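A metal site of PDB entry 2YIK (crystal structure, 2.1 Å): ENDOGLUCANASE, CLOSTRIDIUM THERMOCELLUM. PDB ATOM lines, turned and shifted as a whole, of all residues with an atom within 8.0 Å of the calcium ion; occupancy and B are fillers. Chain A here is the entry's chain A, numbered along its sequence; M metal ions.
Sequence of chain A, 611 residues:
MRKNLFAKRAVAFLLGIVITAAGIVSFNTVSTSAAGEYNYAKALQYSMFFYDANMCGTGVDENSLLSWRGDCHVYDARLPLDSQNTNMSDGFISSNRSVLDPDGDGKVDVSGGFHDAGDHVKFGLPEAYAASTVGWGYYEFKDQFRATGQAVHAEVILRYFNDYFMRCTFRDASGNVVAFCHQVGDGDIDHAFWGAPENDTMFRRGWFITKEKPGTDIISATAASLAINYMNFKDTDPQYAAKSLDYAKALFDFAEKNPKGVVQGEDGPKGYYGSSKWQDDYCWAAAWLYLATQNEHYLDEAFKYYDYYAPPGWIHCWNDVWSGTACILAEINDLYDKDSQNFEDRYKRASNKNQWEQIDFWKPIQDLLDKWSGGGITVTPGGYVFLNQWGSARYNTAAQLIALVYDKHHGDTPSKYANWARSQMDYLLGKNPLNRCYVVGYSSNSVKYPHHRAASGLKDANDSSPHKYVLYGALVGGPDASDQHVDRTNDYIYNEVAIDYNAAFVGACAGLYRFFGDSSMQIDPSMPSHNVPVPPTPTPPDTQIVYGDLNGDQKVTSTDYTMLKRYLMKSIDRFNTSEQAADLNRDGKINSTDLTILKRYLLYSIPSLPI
OD2 of Asp 101 lies within hydrogen-bond range of N of Gly 106, 2.7 Å away. The side-chain carboxylate of Asp 101 sits close to the backbone NH of Gly 104, 3.3 Å away.
The calcium ion is bound by the backbone carbonyl oxygen (O) of Lys 107 (2.4 Å), the side-chain carboxylate (OD1) of Asp 105 (2.5 Å), the side-chain carboxylate (OD1) of Asp 101 (2.6 Å), the side-chain carboxylate (OD1) of Asp 103 (2.6 Å) and the side-chain carboxylate (OD2) of Asp 103 (2.9 Å). The calcium ion has five donor atoms within binding distance.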
ATOM      1  N   ALA A  77      21.787   5.935 -15.212  1.00  0.00           N
ATOM      2  CA  ALA A  77      22.702   6.671 -16.081  1.00  0.00           C
ATOM      3  C   ALA A  77      22.162   8.046 -16.480  1.00  0.00           C
ATOM      4  O   ALA A  77      22.882   8.854 -17.075  1.00  0.00           O
ATOM      5  CB  ALA A  77      23.029   5.844 -17.316  1.00  0.00           C
ATOM      6  N   ARG A  78      20.905   8.307 -16.168  1.00  0.00           N
ATOM      7  CA  ARG A  78      20.274   9.579 -16.485  1.00  0.00           C
ATOM      8  C   ARG A  78      19.507  10.092 -15.282  1.00  0.00           C
ATOM      9  O   ARG A  78      18.347  10.502 -15.405  1.00  0.00           O
ATOM     10  CB  ARG A  78      19.274   9.426 -17.643  1.00  0.00           C
ATOM     11  CG  ARG A  78      19.863   9.031 -18.979  1.00  0.00           C
ATOM     12  CD  ARG A  78      18.917   8.006 -19.606  1.00  0.00           C
ATOM     13  NE  ARG A  78      17.597   8.055 -18.961  1.00  0.00           N
ATOM     14  CZ  ARG A  78      16.714   7.051 -18.963  1.00  0.00           C
ATOM     15  NH1 ARG A  78      17.008   5.903 -19.579  1.00  0.00           N
ATOM     16  NH2 ARG A  78      15.543   7.193 -18.342  1.00  0.00           N
ATOM     17  N   LEU A  79      20.137  10.056 -14.109  1.00  0.00           N
ATOM     18  CA  LEU A  79      19.498  10.536 -12.885  1.00  0.00           C
ATOM     19  C   LEU A  79      19.276  12.045 -12.983  1.00  0.00           C
ATOM     20  O   LEU A  79      20.208  12.795 -13.275  1.00  0.00           O
ATOM     21  CB  LEU A  79      20.394  10.257 -11.685  1.00  0.00           C
ATOM     22  CG  LEU A  79      19.835  10.705 -10.338  1.00  0.00           C
ATOM     23  CD1 LEU A  79      18.622   9.866  -9.989  1.00  0.00           C
ATOM     24  CD2 LEU A  79      20.895  10.564  -9.253  1.00  0.00           C
ATOM     25  N   LEU A  81      19.121  15.806 -12.090  1.00  0.00           N
ATOM     26  CA  LEU A  81      19.847  16.612 -11.135  1.00  0.00           C
ATOM     27  C   LEU A  81      18.944  17.624 -10.426  1.00  0.00           C
ATOM     28  O   LEU A  81      18.782  18.750 -10.892  1.00  0.00           O
ATOM     29  CB  LEU A  81      20.998  17.338 -11.835  1.00  0.00           C
ATOM     30  CG  LEU A  81      21.926  18.233 -10.997  1.00  0.00           C
ATOM     31  CD1 LEU A  81      22.617  17.412  -9.924  1.00  0.00           C
ATOM     32  CD2 LEU A  81      22.949  18.898 -11.907  1.00  0.00           C
ATOM     33  N   ARG A  97      26.419  23.419 -10.517  1.00  0.00           N
ATOM     34  CA  ARG A  97      25.899  22.820 -11.735  1.00  0.00           C
ATOM     35  C   ARG A  97      26.927  22.549 -12.846  1.00  0.00           C
ATOM     36  O   ARG A  97      26.881  21.489 -13.482  1.00  0.00           O
ATOM     37  CB  ARG A  97      24.777  23.702 -12.295  1.00  0.00           C
ATOM     38  CG  ARG A  97      23.953  23.058 -13.380  1.00  0.00           C
ATOM     39  CD  ARG A  97      22.898  24.044 -13.875  1.00  0.00           C
ATOM     40  NE  ARG A  97      22.017  24.469 -12.790  1.00  0.00           N
ATOM     41  CZ  ARG A  97      20.999  23.750 -12.325  1.00  0.00           C
ATOM     42  NH1 ARG A  97      20.726  22.568 -12.865  1.00  0.00           N
ATOM     43  NH2 ARG A  97      20.254  24.200 -11.327  1.00  0.00           N
ATOM     44  N   LEU A 100      28.813  19.406 -11.706  1.00  0.00           N
ATOM     45  CA  LEU A 100      27.947  18.246 -11.575  1.00  0.00           C
ATOM     46  C   LEU A 100      27.338  17.828 -12.910  1.00  0.00           C
ATOM     47  O   LEU A 100      27.074  16.637 -13.130  1.00  0.00           O
ATOM     48  CB  LEU A 100      26.805  18.558 -10.600  1.00  0.00           C
ATOM     49  CG  LEU A 100      27.137  18.841  -9.129  1.00  0.00           C
ATOM     50  CD1 LEU A 100      25.887  19.328  -8.395  1.00  0.00           C
ATOM     51  CD2 LEU A 100      27.676  17.567  -8.478  1.00  0.00           C
ATOM     52  N   ASP A 101      27.124  18.794 -13.799  1.00  0.00           N
ATOM     53  CA  ASP A 101      26.475  18.572 -15.082  1.00  0.00           C
ATOM     54  C   ASP A 101      27.088  19.466 -16.178  1.00  0.00           C
ATOM     55  O   ASP A 101      26.395  20.308 -16.757  1.00  0.00           O
ATOM     56  CB  ASP A 101      24.974  18.853 -14.883  1.00  0.00           C
ATOM     57  CG  ASP A 101      24.146  18.631 -16.130  1.00  0.00           C
ATOM     58  OD1 ASP A 101      24.542  17.809 -16.968  1.00  0.00           O
ATOM     59  OD2 ASP A 101      23.086  19.273 -16.273  1.00  0.00           O
ATOM     60  N   PRO A 102      28.385  19.262 -16.508  1.00  0.00           N
ATOM     61  CA  PRO A 102      29.069  20.066 -17.532  1.00  0.00           C
ATOM     62  C   PRO A 102      28.316  20.220 -18.847  1.00  0.00           C
ATOM     63  O   PRO A 102      28.304  21.301 -19.431  1.00  0.00           O
ATOM     64  CB  PRO A 102      30.397  19.324 -17.729  1.00  0.00           C
ATOM     65  CG  PRO A 102      30.574  18.549 -16.476  1.00  0.00           C
ATOM     66  CD  PRO A 102      29.185  18.072 -16.181  1.00  0.00           C
ATOM     67  N   ASP A 103      27.698  19.136 -19.315  1.00  0.00           N
ATOM     68  CA  ASP A 103      26.980  19.186 -20.588  1.00  0.00           C
ATOM     69  C   ASP A 103      25.612  19.852 -20.501  1.00  0.00           C
ATOM     70  O   ASP A 103      24.970  20.095 -21.526  1.00  0.00           O
ATOM     71  CB  ASP A 103      26.836  17.775 -21.171  1.00  0.00           C
ATOM     72  CG  ASP A 103      26.144  16.839 -20.223  1.00  0.00           C
ATOM     73  OD1 ASP A 103      26.690  16.590 -19.130  1.00  0.00           O
ATOM     74  OD2 ASP A 103      25.045  16.361 -20.553  1.00  0.00           O
ATOM     75  N   GLY A 104      25.171  20.142 -19.288  1.00  0.00           N
ATOM     76  CA  GLY A 104      23.894  20.815 -19.096  1.00  0.00           C
ATOM     77  C   GLY A 104      22.593  20.129 -19.494  1.00  0.00           C
ATOM     78  O   GLY A 104      21.586  20.807 -19.657  1.00  0.00           O
ATOM     79  N   ASP A 105      22.595  18.806 -19.639  1.00  0.00           N
ATOM     80  CA  ASP A 105      21.355  18.142 -20.018  1.00  0.00           C
ATOM     81  C   ASP A 105      20.472  17.848 -18.791  1.00  0.00           C
ATOM     82  O   ASP A 105      19.432  17.191 -18.901  1.00  0.00           O
ATOM     83  CB  ASP A 105      21.635  16.849 -20.794  1.00  0.00           C
ATOM     84  CG  ASP A 105      22.090  15.705 -19.892  1.00  0.00           C
ATOM     85  OD1 ASP A 105      22.359  15.963 -18.707  1.00  0.00           O
ATOM     86  OD2 ASP A 105      22.175  14.557 -20.369  1.00  0.00           O
ATOM     87  N   GLY A 106      20.895  18.340 -17.635  1.00  0.00           N
ATOM     88  CA  GLY A 106      20.139  18.155 -16.401  1.00  0.00           C
ATOM     89  C   GLY A 106      20.103  16.760 -15.806  1.00  0.00           C
ATOM     90  O   GLY A 106      19.260  16.465 -14.956  1.00  0.00           O
ATOM     91  N   LYS A 107      21.012  15.894 -16.240  1.00  0.00           N
ATOM     92  CA  LYS A 107      21.060  14.534 -15.733  1.00  0.00           C
ATOM     93  C   LYS A 107      22.488  14.118 -15.410  1.00  0.00           C
ATOM     94  O   LYS A 107      23.436  14.639 -15.969  1.00  0.00           O
ATOM     95  CB  LYS A 107      20.457  13.583 -16.773  1.00  0.00           C
ATOM     96  CG  LYS A 107      18.947  13.751 -16.933  1.00  0.00           C
ATOM     97  CD  LYS A 107      18.513  13.560 -18.373  1.00  0.00           C
ATOM     98  CE  LYS A 107      16.987  13.561 -18.518  1.00  0.00           C
ATOM     99  NZ  LYS A 107      16.310  14.135 -17.313  1.00  0.00           N
ATOM    100  N   VAL A 108      22.665  13.192 -14.474  1.00  0.00           N
ATOM    101  CA  VAL A 108      24.006  12.713 -14.167  1.00  0.00           C
ATOM    102  C   VAL A 108      24.001  11.205 -14.272  1.00  0.00           C
ATOM    103  O   VAL A 108      22.960  10.565 -14.131  1.00  0.00           O
ATOM    104  CB  VAL A 108      24.477  13.141 -12.758  1.00  0.00           C
ATOM    105  CG1 VAL A 108      24.552  14.661 -12.667  1.00  0.00           C
ATOM    106  CG2 VAL A 108      23.537  12.575 -11.708  1.00  0.00           C
ATOM    107  N   ASP A 109      25.176  10.631 -14.527  1.00  0.00           N
ATOM    108  CA  ASP A 109      25.318   9.193 -14.674  1.00  0.00           C
ATOM    109  C   ASP A 109      25.920   8.536 -13.420  1.00  0.00           C
ATOM    110  O   ASP A 109      27.118   8.659 -13.169  1.00  0.00           O
ATOM    111  CB  ASP A 109      26.192   8.896 -15.894  1.00  0.00           C
ATOM    112  CG  ASP A 109      26.341   7.410 -16.169  1.00  0.00           C
ATOM    113  OD1 ASP A 109      25.783   6.578 -15.413  1.00  0.00           O
ATOM    114  OD2 ASP A 109      27.037   7.064 -17.153  1.00  0.00           O
ATOM    115  N   PHE A 170      32.477  13.544  -8.565  1.00  0.00           N
ATOM    116  CA  PHE A 170      32.376  14.777  -9.349  1.00  0.00           C
ATOM    117  C   PHE A 170      33.432  15.771  -8.847  1.00  0.00           C
ATOM    118  O   PHE A 170      33.334  16.286  -7.732  1.00  0.00           O
ATOM    119  CB  PHE A 170      30.962  15.331  -9.222  1.00  0.00           C
ATOM    120  CG  PHE A 170      29.904  14.396  -9.739  1.00  0.00           C
ATOM    121  CD1 PHE A 170      29.415  13.368  -8.931  1.00  0.00           C
ATOM    122  CD2 PHE A 170      29.476  14.471 -11.058  1.00  0.00           C
ATOM    123  CE1 PHE A 170      28.519  12.438  -9.436  1.00  0.00           C
ATOM    124  CE2 PHE A 170      28.569  13.548 -11.566  1.00  0.00           C
ATOM    125  CZ  PHE A 170      28.096  12.521 -10.756  1.00  0.00           C
HETATM  126 CA    CA M   1      24.687  15.414 -17.867  1.00  0.00          CA
